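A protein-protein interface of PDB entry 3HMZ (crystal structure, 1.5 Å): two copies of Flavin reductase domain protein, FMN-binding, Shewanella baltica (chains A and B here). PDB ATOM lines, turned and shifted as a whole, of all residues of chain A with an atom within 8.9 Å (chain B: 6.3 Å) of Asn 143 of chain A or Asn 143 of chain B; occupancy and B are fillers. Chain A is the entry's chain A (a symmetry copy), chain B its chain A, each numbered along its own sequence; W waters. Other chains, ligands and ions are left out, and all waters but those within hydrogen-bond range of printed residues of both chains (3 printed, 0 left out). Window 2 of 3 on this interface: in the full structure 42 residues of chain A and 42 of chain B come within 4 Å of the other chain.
OD1 of Asn 143 of chain B is in hydrogen-bond range of ND2 of Asn 143 of chain A (2.9 Å). The side-chain hydroxyl (OH) of Tyr 147 of chain B sits at hydrogen-bond distance from the side-chain carboxylate (OE2) of Glu 140 of chain A, at 2.6 Å. OH of Tyr 147 of chain A sits at hydrogen-bond distance from OE2 of Glu 140 of chain B (2.6 Å).
N of Asp 148 of chain A lies within hydrogen-bond range of O of Asn 143 of chain A, at 3.1 Å. The backbone NH of Leu 149 of chain B lies within hydrogen-bond range of the backbone carbonyl oxygen of Asn 143 of chain B (3.2 Å). The backbone carbonyl oxygen (O) of Asn 143 of chain B lies within hydrogen-bond range of the backbone NH (N) of Asp 148 of chain B (3.1 Å). The backbone carbonyl oxygen of Asn 143 of chain A sits at hydrogen-bond distance from the backbone NH of Leu 149 of chain A (3.2 Å). N of Glu 140 of chain A sits at hydrogen-bond distance from OE1 of Gln 144 of chain A (3.0 Å). N of Glu 140 of chain B lies within hydrogen-bond range of OE1 of Gln 144 of chain B, 3.0 Å away.
Tyr 147 of chain B touches Leu 53 of chain A (O to CD1, 3.6 Å). Ile 138 of chain A touches Tyr 147 of chain B (CG2 to OH, 3.3 Å). CD1 of Ile 151 of chain B touches CE2 of Tyr 147 of chain A (3.6 Å). Tyr 147 of chain B touches Ile 151 of chain A.
Of the printed residues of chain B, Asn 143 of chain A touches Asn 143. Of chain A, only Asn 143 (2.9 Å) comes within 4 Å of Asn 143 of chain B. No residue of chain A comes within 4 Å of Asn 142 of chain B. Printed residues of chain A within 4 Å of Glu 140 of chain B: Tyr 147 (2.6 Å). Of the printed residues of chain A, Tyr 147 of chain B touches Leu 53, Ile 138, Glu 140 and Ile 151. Asn 142 of chain A touches none of the printed residues of chain B. The nearest residue of chain B that does not touch Asn 143 of chain A is Ile 151 of chain B (4.8 Å). The nearest residue of chain A that does not touch Asn 143 of chain B is Ile 151 of chain A (4.8 Å). The nearest printed residue of chain A that does not touch Glu 140 of chain B is Asn 142 of chain A (4.04 Å).
Hydrophobic or aromatic side chains of chain B within 4 Å of the printed part of chain A: Tyr 147 and Ile 151.
Glu 140 of chain A touches Tyr 147 of chain B, and with the chains exchanged Tyr 147 of chain A touches Glu 140 of chain B. Asn 143 of chain B touches its own counterpart, Asn 143 of chain A. Tyr 147 of chain A touches Ile 151 of chain B, and with the chains exchanged Ile 151 of chain A touches Tyr 147 of chain B. 12 positions are printed for both chains.
Water W3 bridges O of Leu 53 of chain A (2.7 Å) and O of Tyr 147 of chain B (2.8 Å). Water W2 lies within hydrogen-bond range of OD1 of Asn 143 of chain B (2.7 Å), ND2 of Asn 142 of chain B (2.8 Å) and OE1 of Glu 140 of chain A (3.2 Å). Water W1 lies within hydrogen-bond range of OD1 of Asn 143 of chain A (2.7 Å), ND2 of Asn 142 of chain A (2.7 Å) and OE1 of Glu 140 of chain B (3.2 Å).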
ATOM      1  N   LEU A  53      -8.974  18.657 -12.105  1.00  0.00           N
ATOM      2  CA  LEU A  53      -7.815  19.321 -12.738  1.00  0.00           C
ATOM      3  C   LEU A  53      -8.195  20.185 -13.934  1.00  0.00           C
ATOM      4  O   LEU A  53      -7.502  21.190 -14.198  1.00  0.00           O
ATOM      5  CB  LEU A  53      -6.756  18.286 -13.139  1.00  0.00           C
ATOM      6  CG  LEU A  53      -5.506  18.777 -13.866  1.00  0.00           C
ATOM      7  CD1 LEU A  53      -4.791  19.762 -12.964  1.00  0.00           C
ATOM      8  CD2 LEU A  53      -4.611  17.555 -14.264  1.00  0.00           C
ATOM      9  N   THR A  61      -6.653  14.696 -10.806  1.00  0.00           N
ATOM     10  CA  THR A  61      -5.456  14.199 -10.191  1.00  0.00           C
ATOM     11  C   THR A  61      -5.839  13.216  -9.101  1.00  0.00           C
ATOM     12  O   THR A  61      -6.896  13.365  -8.468  1.00  0.00           O
ATOM     13  CB  THR A  61      -4.559  15.305  -9.567  1.00  0.00           C
ATOM     14  OG1 THR A  61      -5.329  16.067  -8.621  1.00  0.00           O
ATOM     15  CG2 THR A  61      -3.963  16.216 -10.671  1.00  0.00           C
ATOM     16  N   VAL A  62      -4.954  12.258  -8.819  1.00  0.00           N
ATOM     17  CA  VAL A  62      -5.079  11.398  -7.634  1.00  0.00           C
ATOM     18  C   VAL A  62      -3.669  11.030  -7.154  1.00  0.00           C
ATOM     19  O   VAL A  62      -2.759  10.841  -7.972  1.00  0.00           O
ATOM     20  CB  VAL A  62      -5.988  10.182  -7.863  1.00  0.00           C
ATOM     21  CG1 VAL A  62      -5.432   9.199  -8.964  1.00  0.00           C
ATOM     22  CG2 VAL A  62      -6.288   9.512  -6.538  1.00  0.00           C
ATOM     23  N   VAL A  63      -3.493  11.015  -5.853  1.00  0.00           N
ATOM     24  CA  VAL A  63      -2.240  10.647  -5.215  1.00  0.00           C
ATOM     25  C   VAL A  63      -2.356   9.191  -4.806  1.00  0.00           C
ATOM     26  O   VAL A  63      -3.269   8.814  -4.060  1.00  0.00           O
ATOM     27  CB  VAL A  63      -1.926  11.545  -4.022  1.00  0.00           C
ATOM     28  CG1 VAL A  63      -0.558  11.194  -3.484  1.00  0.00           C
ATOM     29  CG2 VAL A  63      -2.001  13.029  -4.432  1.00  0.00           C
ATOM     30  N   LEU A  64      -1.439   8.358  -5.303  1.00  0.00           N
ATOM     31  CA  LEU A  64      -1.462   6.910  -5.044  1.00  0.00           C
ATOM     32  C   LEU A  64      -0.132   6.483  -4.453  1.00  0.00           C
ATOM     33  O   LEU A  64       0.898   6.533  -5.118  1.00  0.00           O
ATOM     34  CB  LEU A  64      -1.736   6.148  -6.322  1.00  0.00           C
ATOM     35  CG  LEU A  64      -3.000   6.521  -7.106  1.00  0.00           C
ATOM     36  CD1 LEU A  64      -2.993   5.841  -8.501  1.00  0.00           C
ATOM     37  CD2 LEU A  64      -4.247   6.209  -6.314  1.00  0.00           C
ATOM     38  N   LYS A  66       3.026   4.382  -3.292  1.00  0.00           N
ATOM     39  CA  LYS A  66       3.775   3.280  -3.891  1.00  0.00           C
ATOM     40  C   LYS A  66       3.458   1.886  -3.312  1.00  0.00           C
ATOM     41  O   LYS A  66       3.727   0.903  -3.991  1.00  0.00           O
ATOM     42  CB  LYS A  66       5.289   3.545  -3.774  1.00  0.00           C
ATOM     43  CG  LYS A  66       5.729   4.685  -4.655  1.00  0.00           C
ATOM     44  CD  LYS A  66       7.258   4.851  -4.638  1.00  0.00           C
ATOM     45  CE  LYS A  66       7.729   5.970  -5.539  1.00  0.00           C
ATOM     46  NZ  LYS A  66       7.420   7.326  -5.047  1.00  0.00           N
ATOM     47  N   ARG A  71      -2.351   1.134  -7.293  1.00  0.00           N
ATOM     48  CA  ARG A  71      -1.383   1.876  -8.112  1.00  0.00           C
ATOM     49  C   ARG A  71      -0.734   0.961  -9.165  1.00  0.00           C
ATOM     50  O   ARG A  71      -0.587   1.339 -10.341  1.00  0.00           O
ATOM     51  CB  ARG A  71      -0.322   2.496  -7.236  1.00  0.00           C
ATOM     52  CG  ARG A  71       0.794   3.119  -8.028  1.00  0.00           C
ATOM     53  CD  ARG A  71       1.704   3.852  -7.140  1.00  0.00           C
ATOM     54  NE  ARG A  71       2.908   4.279  -7.871  1.00  0.00           N
ATOM     55  CZ  ARG A  71       3.628   5.362  -7.609  1.00  0.00           C
ATOM     56  NH1 ARG A  71       3.264   6.209  -6.637  1.00  0.00           N
ATOM     57  NH2 ARG A  71       4.722   5.636  -8.346  1.00  0.00           N
ATOM     58  N   LEU A 137      -5.388   7.235 -17.780  1.00  0.00           N
ATOM     59  CA  LEU A 137      -4.131   7.797 -17.320  1.00  0.00           C
ATOM     60  C   LEU A 137      -3.385   8.554 -18.426  1.00  0.00           C
ATOM     61  O   LEU A 137      -3.308   8.091 -19.555  1.00  0.00           O
ATOM     62  CB  LEU A 137      -3.202   6.693 -16.778  1.00  0.00           C
ATOM     63  CG  LEU A 137      -1.853   7.092 -16.153  1.00  0.00           C
ATOM     64  CD1 LEU A 137      -2.058   7.943 -14.875  1.00  0.00           C
ATOM     65  CD2 LEU A 137      -0.975   5.859 -15.896  1.00  0.00           C
ATOM     66  N   ILE A 138      -2.868   9.717 -18.078  1.00  0.00           N
ATOM     67  CA  ILE A 138      -1.927  10.481 -18.922  1.00  0.00           C
ATOM     68  C   ILE A 138      -0.567  10.243 -18.255  1.00  0.00           C
ATOM     69  O   ILE A 138      -0.268  10.872 -17.240  1.00  0.00           O
ATOM     70  CB  ILE A 138      -2.250  11.964 -18.974  1.00  0.00           C
ATOM     71  CG1 ILE A 138      -3.639  12.185 -19.536  1.00  0.00           C
ATOM     72  CG2 ILE A 138      -1.134  12.705 -19.844  1.00  0.00           C
ATOM     73  CD1 ILE A 138      -4.095  13.608 -19.470  1.00  0.00           C
ATOM     74  N   PRO A 139       0.273   9.330 -18.797  1.00  0.00           N
ATOM     75  CA  PRO A 139       1.506   9.004 -18.077  1.00  0.00           C
ATOM     76  C   PRO A 139       2.454  10.182 -17.890  1.00  0.00           C
ATOM     77  O   PRO A 139       2.708  10.913 -18.843  1.00  0.00           O
ATOM     78  CB  PRO A 139       2.139   7.905 -18.954  1.00  0.00           C
ATOM     79  CG  PRO A 139       0.993   7.315 -19.692  1.00  0.00           C
ATOM     80  CD  PRO A 139       0.088   8.467 -19.985  1.00  0.00           C
ATOM     81  N   GLU A 140       2.909  10.378 -16.653  1.00  0.00           N
ATOM     82  CA  GLU A 140       3.808  11.465 -16.269  1.00  0.00           C
ATOM     83  C   GLU A 140       4.826  10.851 -15.347  1.00  0.00           C
ATOM     84  O   GLU A 140       4.671  10.882 -14.134  1.00  0.00           O
ATOM     85  CB  GLU A 140       3.006  12.598 -15.616  1.00  0.00           C
ATOM     86  CG  GLU A 140       2.139  13.397 -16.562  1.00  0.00           C
ATOM     87  CD  GLU A 140       2.904  14.314 -17.486  1.00  0.00           C
ATOM     88  OE1 GLU A 140       4.120  14.525 -17.248  1.00  0.00           O
ATOM     89  OE2 GLU A 140       2.307  14.806 -18.457  1.00  0.00           O
ATOM     90  N   PRO A 141       5.918  10.248 -15.914  1.00  0.00           N
ATOM     91  CA  PRO A 141       6.865   9.552 -15.062  1.00  0.00           C
ATOM     92  C   PRO A 141       7.410  10.286 -13.860  1.00  0.00           C
ATOM     93  O   PRO A 141       7.449   9.721 -12.785  1.00  0.00           O
ATOM     94  CB  PRO A 141       8.005   9.180 -16.031  1.00  0.00           C
ATOM     95  CG  PRO A 141       7.299   9.041 -17.325  1.00  0.00           C
ATOM     96  CD  PRO A 141       6.238  10.099 -17.346  1.00  0.00           C
ATOM     97  N   ASN A 142       7.808  11.546 -14.027  1.00  0.00           N
ATOM     98  CA  ASN A 142       8.396  12.299 -12.928  1.00  0.00           C
ATOM     99  C   ASN A 142       7.386  12.569 -11.817  1.00  0.00           C
ATOM    100  O   ASN A 142       7.685  12.381 -10.649  1.00  0.00           O
ATOM    101  CB  ASN A 142       8.970  13.630 -13.395  1.00  0.00           C
ATOM    102  CG  ASN A 142       9.819  14.264 -12.318  1.00  0.00           C
ATOM    103  OD1 ASN A 142      10.817  13.686 -11.908  1.00  0.00           O
ATOM    104  ND2 ASN A 142       9.380  15.395 -11.792  1.00  0.00           N
ATOM    105  N   ASN A 143       6.187  12.982 -12.202  1.00  0.00           N
ATOM    106  CA  ASN A 143       5.144  13.231 -11.180  1.00  0.00           C
ATOM    107  C   ASN A 143       4.839  11.958 -10.395  1.00  0.00           C
ATOM    108  O   ASN A 143       4.697  11.980  -9.163  1.00  0.00           O
ATOM    109  CB  ASN A 143       3.828  13.697 -11.807  1.00  0.00           C
ATOM    110  CG  ASN A 143       3.826  15.134 -12.243  1.00  0.00           C
ATOM    111  OD1 ASN A 143       4.665  15.929 -11.829  1.00  0.00           O
ATOM    112  ND2 ASN A 143       2.812  15.495 -13.043  1.00  0.00           N
ATOM    113  N   GLN A 144       4.759  10.845 -11.119  1.00  0.00           N
ATOM    114  CA  GLN A 144       4.394   9.580 -10.477  1.00  0.00           C
ATOM    115  C   GLN A 144       5.474   9.055  -9.523  1.00  0.00           C
ATOM    116  O   GLN A 144       5.190   8.527  -8.436  1.00  0.00           O
ATOM    117  CB  GLN A 144       3.994   8.554 -11.543  1.00  0.00           C
ATOM    118  CG  GLN A 144       2.709   8.947 -12.274  1.00  0.00           C
ATOM    119  CD  GLN A 144       2.432   8.190 -13.565  1.00  0.00           C
ATOM    120  OE1 GLN A 144       1.802   8.731 -14.469  1.00  0.00           O
ATOM    121  NE2 GLN A 144       2.920   6.940 -13.662  1.00  0.00           N
ATOM    122  N   LEU A 145       6.744   9.241  -9.915  1.00  0.00           N
ATOM    123  CA  LEU A 145       7.850   8.790  -9.088  1.00  0.00           C
ATOM    124  C   LEU A 145       8.143   9.727  -7.922  1.00  0.00           C
ATOM    125  O   LEU A 145       8.254   9.285  -6.755  1.00  0.00           O
ATOM    126  CB  LEU A 145       9.120   8.682  -9.970  1.00  0.00           C
ATOM    127  CG  LEU A 145      10.376   8.154  -9.257  1.00  0.00           C
ATOM    128  CD1 LEU A 145      10.171   6.777  -8.663  1.00  0.00           C
ATOM    129  CD2 LEU A 145      11.574   8.197 -10.269  1.00  0.00           C
ATOM    130  N   GLN A 146       8.260  11.015  -8.246  1.00  0.00           N
ATOM    131  CA  GLN A 146       8.635  12.036  -7.252  1.00  0.00           C
ATOM    132  C   GLN A 146       7.532  12.403  -6.265  1.00  0.00           C
ATOM    133  O   GLN A 146       7.800  12.597  -5.096  1.00  0.00           O
ATOM    134  CB  GLN A 146       9.131  13.310  -7.944  1.00  0.00           C
ATOM    135  CG  GLN A 146      10.369  13.094  -8.802  1.00  0.00           C
ATOM    136  CD  GLN A 146      11.497  12.500  -8.017  1.00  0.00           C
ATOM    137  OE1 GLN A 146      11.687  12.820  -6.855  1.00  0.00           O
ATOM    138  NE2 GLN A 146      12.260  11.626  -8.659  1.00  0.00           N
ATOM    139  N   TYR A 147       6.291  12.465  -6.759  1.00  0.00           N
ATOM    140  CA  TYR A 147       5.146  12.912  -5.948  1.00  0.00           C
ATOM    141  C   TYR A 147       4.021  11.929  -5.827  1.00  0.00           C
ATOM    142  O   TYR A 147       3.012  12.278  -5.232  1.00  0.00           O
ATOM    143  CB  TYR A 147       4.594  14.203  -6.575  1.00  0.00           C
ATOM    144  CG  TYR A 147       5.601  15.324  -6.710  1.00  0.00           C
ATOM    145  CD1 TYR A 147       6.106  15.953  -5.584  1.00  0.00           C
ATOM    146  CD2 TYR A 147       5.999  15.779  -7.963  1.00  0.00           C
ATOM    147  CE1 TYR A 147       7.066  16.970  -5.703  1.00  0.00           C
ATOM    148  CE2 TYR A 147       6.930  16.818  -8.095  1.00  0.00           C
ATOM    149  CZ  TYR A 147       7.434  17.418  -6.960  1.00  0.00           C
ATOM    150  OH  TYR A 147       8.328  18.473  -7.079  1.00  0.00           O
ATOM    151  N   ASP A 148       4.131  10.721  -6.386  1.00  0.00           N
ATOM    152  CA  ASP A 148       2.995   9.756  -6.317  1.00  0.00           C
ATOM    153  C   ASP A 148       1.722  10.364  -6.915  1.00  0.00           C
ATOM    154  O   ASP A 148       0.623   9.987  -6.566  1.00  0.00           O
ATOM    155  CB  ASP A 148       2.783   9.272  -4.866  1.00  0.00           C
ATOM    156  CG  ASP A 148       3.997   8.580  -4.313  1.00  0.00           C
ATOM    157  OD1 ASP A 148       4.713   7.949  -5.141  1.00  0.00           O
ATOM    158  OD2 ASP A 148       4.255   8.703  -3.096  1.00  0.00           O
ATOM    159  N   LEU A 149       1.887  11.278  -7.863  1.00  0.00           N
ATOM    160  CA  LEU A 149       0.791  12.096  -8.412  1.00  0.00           C
ATOM    161  C   LEU A 149       0.460  11.638  -9.811  1.00  0.00           C
ATOM    162  O   LEU A 149       1.308  11.694 -10.718  1.00  0.00           O
ATOM    163  CB  LEU A 149       1.234  13.546  -8.404  1.00  0.00           C
ATOM    164  CG  LEU A 149       0.296  14.631  -8.925  1.00  0.00           C
ATOM    165  CD1 LEU A 149      -1.014  14.616  -8.106  1.00  0.00           C
ATOM    166  CD2 LEU A 149       0.975  15.979  -8.918  1.00  0.00           C
ATOM    167  N   PHE A 150      -0.799  11.249  -9.997  1.00  0.00           N
ATOM    168  CA  PHE A 150      -1.301  10.705 -11.228  1.00  0.00           C
ATOM    169  C   PHE A 150      -2.336  11.639 -11.817  1.00  0.00           C
ATOM    170  O   PHE A 150      -3.144  12.180 -11.079  1.00  0.00           O
ATOM    171  CB  PHE A 150      -1.907   9.315 -10.962  1.00  0.00           C
ATOM    172  CG  PHE A 150      -0.878   8.282 -10.596  1.00  0.00           C
ATOM    173  CD1 PHE A 150      -0.291   8.256  -9.369  1.00  0.00           C
ATOM    174  CD2 PHE A 150      -0.512   7.312 -11.530  1.00  0.00           C
ATOM    175  CE1 PHE A 150       0.700   7.343  -9.050  1.00  0.00           C
ATOM    176  CE2 PHE A 150       0.454   6.354 -11.215  1.00  0.00           C
ATOM    177  CZ  PHE A 150       1.071   6.375  -9.991  1.00  0.00           C
ATOM    178  N   ILE A 151      -2.266  11.863 -13.118  1.00  0.00           N
ATOM    179  CA  ILE A 151      -3.173  12.705 -13.900  1.00  0.00           C
ATOM    180  C   ILE A 151      -3.931  11.837 -14.866  1.00  0.00           C
ATOM    181  O   ILE A 151      -3.330  10.985 -15.547  1.00  0.00           O
ATOM    182  CB  ILE A 151      -2.377  13.811 -14.664  1.00  0.00           C
ATOM    183  CG1 ILE A 151      -1.811  14.811 -13.648  1.00  0.00           C
ATOM    184  CG2 ILE A 151      -3.274  14.528 -15.687  1.00  0.00           C
ATOM    185  CD1 ILE A 151      -0.811  15.783 -14.249  1.00  0.00           C
ATOM    186  N   GLU B 140       7.791  23.580 -11.008  1.00  0.00           N
ATOM    187  CA  GLU B 140       7.628  22.443 -11.914  1.00  0.00           C
ATOM    188  C   GLU B 140       7.150  23.020 -13.218  1.00  0.00           C
ATOM    189  O   GLU B 140       5.956  23.081 -13.476  1.00  0.00           O
ATOM    190  CB  GLU B 140       6.649  21.430 -11.306  1.00  0.00           C
ATOM    191  CG  GLU B 140       7.182  20.653 -10.125  1.00  0.00           C
ATOM    192  CD  GLU B 140       8.220  19.615 -10.477  1.00  0.00           C
ATOM    193  OE1 GLU B 140       8.377  19.312 -11.686  1.00  0.00           O
ATOM    194  OE2 GLU B 140       8.894  19.118  -9.559  1.00  0.00           O
ATOM    195  N   PRO B 141       8.096  23.488 -14.093  1.00  0.00           N
ATOM    196  CA  PRO B 141       7.668  24.148 -15.313  1.00  0.00           C
ATOM    197  C   PRO B 141       6.651  23.446 -16.180  1.00  0.00           C
ATOM    198  O   PRO B 141       5.704  24.072 -16.612  1.00  0.00           O
ATOM    199  CB  PRO B 141       8.987  24.355 -16.084  1.00  0.00           C
ATOM    200  CG  PRO B 141       9.984  24.474 -14.995  1.00  0.00           C
ATOM    201  CD  PRO B 141       9.560  23.516 -13.924  1.00  0.00           C
ATOM    202  N   ASN B 142       6.827  22.147 -16.420  1.00  0.00           N
ATOM    203  CA  ASN B 142       5.920  21.415 -17.293  1.00  0.00           C
ATOM    204  C   ASN B 142       4.519  21.307 -16.698  1.00  0.00           C
ATOM    205  O   ASN B 142       3.536  21.542 -17.382  1.00  0.00           O
ATOM    206  CB  ASN B 142       6.428  20.012 -17.592  1.00  0.00           C
ATOM    207  CG  ASN B 142       5.638  19.374 -18.710  1.00  0.00           C
ATOM    208  OD1 ASN B 142       5.631  19.885 -19.823  1.00  0.00           O
ATOM    209  ND2 ASN B 142       4.898  18.322 -18.403  1.00  0.00           N
ATOM    210  N   ASN B 143       4.450  20.980 -15.416  1.00  0.00           N
ATOM    211  CA  ASN B 143       3.123  20.890 -14.761  1.00  0.00           C
ATOM    212  C   ASN B 143       2.399  22.232 -14.817  1.00  0.00           C
ATOM    213  O   ASN B 143       1.193  22.300 -15.095  1.00  0.00           O
ATOM    214  CB  ASN B 143       3.239  20.504 -13.284  1.00  0.00           C
ATOM    215  CG  ASN B 143       3.520  19.048 -13.045  1.00  0.00           C
ATOM    216  OD1 ASN B 143       3.336  18.210 -13.923  1.00  0.00           O
ATOM    217  ND2 ASN B 143       3.908  18.729 -11.802  1.00  0.00           N
ATOM    218  N   GLN B 144       3.153  23.299 -14.570  1.00  0.00           N
ATOM    219  CA  GLN B 144       2.542  24.630 -14.522  1.00  0.00           C
ATOM    220  C   GLN B 144       2.047  25.115 -15.889  1.00  0.00           C
ATOM    221  O   GLN B 144       0.979  25.734 -16.020  1.00  0.00           O
ATOM    222  CB  GLN B 144       3.505  25.619 -13.854  1.00  0.00           C
ATOM    223  CG  GLN B 144       3.735  25.296 -12.376  1.00  0.00           C
ATOM    224  CD  GLN B 144       4.925  25.992 -11.732  1.00  0.00           C
ATOM    225  OE1 GLN B 144       5.520  25.453 -10.803  1.00  0.00           O
ATOM    226  NE2 GLN B 144       5.288  27.185 -12.236  1.00  0.00           N
ATOM    227  N   LEU B 145       2.816  24.794 -16.941  1.00  0.00           N
ATOM    228  CA  LEU B 145       2.444  25.195 -18.286  1.00  0.00           C
ATOM    229  C   LEU B 145       1.359  24.311 -18.892  1.00  0.00           C
ATOM    230  O   LEU B 145       0.338  24.814 -19.416  1.00  0.00           O
ATOM    231  CB  LEU B 145       3.698  25.133 -19.192  1.00  0.00           C
ATOM    232  CG  LEU B 145       3.488  25.591 -20.644  1.00  0.00           C
ATOM    233  CD1 LEU B 145       2.986  27.016 -20.737  1.00  0.00           C
ATOM    234  CD2 LEU B 145       4.829  25.377 -21.430  1.00  0.00           C
ATOM    235  N   GLN B 146       1.587  23.000 -18.813  1.00  0.00           N
ATOM    236  CA  GLN B 146       0.685  22.014 -19.433  1.00  0.00           C
ATOM    237  C   GLN B 146      -0.638  21.810 -18.703  1.00  0.00           C
ATOM    238  O   GLN B 146      -1.667  21.667 -19.334  1.00  0.00           O
ATOM    239  CB  GLN B 146       1.384  20.660 -19.588  1.00  0.00           C
ATOM    240  CG  GLN B 146       2.618  20.710 -20.478  1.00  0.00           C
ATOM    241  CD  GLN B 146       2.303  21.249 -21.839  1.00  0.00           C
ATOM    242  OE1 GLN B 146       1.245  20.987 -22.387  1.00  0.00           O
ATOM    243  NE2 GLN B 146       3.236  22.009 -22.397  1.00  0.00           N
ATOM    244  N   TYR B 147      -0.588  21.828 -17.367  1.00  0.00           N
ATOM    245  CA  TYR B 147      -1.766  21.537 -16.534  1.00  0.00           C
ATOM    246  C   TYR B 147      -2.161  22.622 -15.579  1.00  0.00           C
ATOM    247  O   TYR B 147      -3.085  22.403 -14.806  1.00  0.00           O
ATOM    248  CB  TYR B 147      -1.474  20.263 -15.724  1.00  0.00           C
ATOM    249  CG  TYR B 147      -1.115  19.051 -16.554  1.00  0.00           C
ATOM    250  CD1 TYR B 147      -2.064  18.452 -17.366  1.00  0.00           C
ATOM    251  CD2 TYR B 147       0.153  18.483 -16.481  1.00  0.00           C
ATOM    252  CE1 TYR B 147      -1.727  17.348 -18.164  1.00  0.00           C
ATOM    253  CE2 TYR B 147       0.491  17.360 -17.246  1.00  0.00           C
ATOM    254  CZ  TYR B 147      -0.465  16.790 -18.063  1.00  0.00           C
ATOM    255  OH  TYR B 147      -0.153  15.654 -18.797  1.00  0.00           O
ATOM    256  N   ASP B 148      -1.492  23.778 -15.571  1.00  0.00           N
ATOM    257  CA  ASP B 148      -1.845  24.843 -14.587  1.00  0.00           C
ATOM    258  C   ASP B 148      -1.756  24.314 -13.151  1.00  0.00           C
ATOM    259  O   ASP B 148      -2.411  24.809 -12.259  1.00  0.00           O
ATOM    260  CB  ASP B 148      -3.235  25.434 -14.904  1.00  0.00           C
ATOM    261  CG  ASP B 148      -3.294  26.049 -16.274  1.00  0.00           C
ATOM    262  OD1 ASP B 148      -2.225  26.560 -16.710  1.00  0.00           O
ATOM    263  OD2 ASP B 148      -4.364  25.980 -16.916  1.00  0.00           O
ATOM    264  N   LEU B 149      -0.891  23.331 -12.932  1.00  0.00           N
ATOM    265  CA  LEU B 149      -0.808  22.581 -11.666  1.00  0.00           C
ATOM    266  C   LEU B 149       0.439  22.978 -10.916  1.00  0.00           C
ATOM    267  O   LEU B 149       1.567  22.788 -11.406  1.00  0.00           O
ATOM    268  CB  LEU B 149      -0.799  21.101 -11.994  1.00  0.00           C
ATOM    269  CG  LEU B 149      -0.715  20.073 -10.869  1.00  0.00           C
ATOM    270  CD1 LEU B 149      -1.914  20.256  -9.913  1.00  0.00           C
ATOM    271  CD2 LEU B 149      -0.618  18.674 -11.424  1.00  0.00           C
ATOM    272  N   PHE B 150       0.235  23.464  -9.695  1.00  0.00           N
ATOM    273  CA  PHE B 150       1.277  23.973  -8.844  1.00  0.00           C
ATOM    274  C   PHE B 150       1.407  23.099  -7.615  1.00  0.00           C
ATOM    275  O   PHE B 150       0.399  22.680  -7.069  1.00  0.00           O
ATOM    276  CB  PHE B 150       0.951  25.425  -8.452  1.00  0.00           C
ATOM    277  CG  PHE B 150       1.038  26.383  -9.607  1.00  0.00           C
ATOM    278  CD1 PHE B 150       0.079  26.434 -10.572  1.00  0.00           C
ATOM    279  CD2 PHE B 150       2.123  27.256  -9.700  1.00  0.00           C
ATOM    280  CE1 PHE B 150       0.186  27.273 -11.668  1.00  0.00           C
ATOM    281  CE2 PHE B 150       2.229  28.142 -10.774  1.00  0.00           C
ATOM    282  CZ  PHE B 150       1.280  28.143 -11.763  1.00  0.00           C
ATOM    283  N   ILE B 151       2.634  22.788  -7.232  1.00  0.00           N
ATOM    284  CA  ILE B 151       2.995  21.984  -6.064  1.00  0.00           C
ATOM    285  C   ILE B 151       3.732  22.853  -5.082  1.00  0.00           C
ATOM    286  O   ILE B 151       4.646  23.602  -5.475  1.00  0.00           O
ATOM    287  CB  ILE B 151       3.877  20.764  -6.488  1.00  0.00           C
ATOM    288  CG1 ILE B 151       3.018  19.784  -7.297  1.00  0.00           C
ATOM    289  CG2 ILE B 151       4.480  20.067  -5.256  1.00  0.00           C
ATOM    290  CD1 ILE B 151       3.825  18.690  -7.974  1.00  0.00           C
HETATM  291  O   HOH W   1       7.125  16.622 -12.777  1.00  0.00           O
HETATM  292  O   HOH W   2       4.974  17.242 -15.875  1.00  0.00           O
HETATM  293  O   HOH W   3      -5.591  21.937 -15.891  1.00  0.00           O
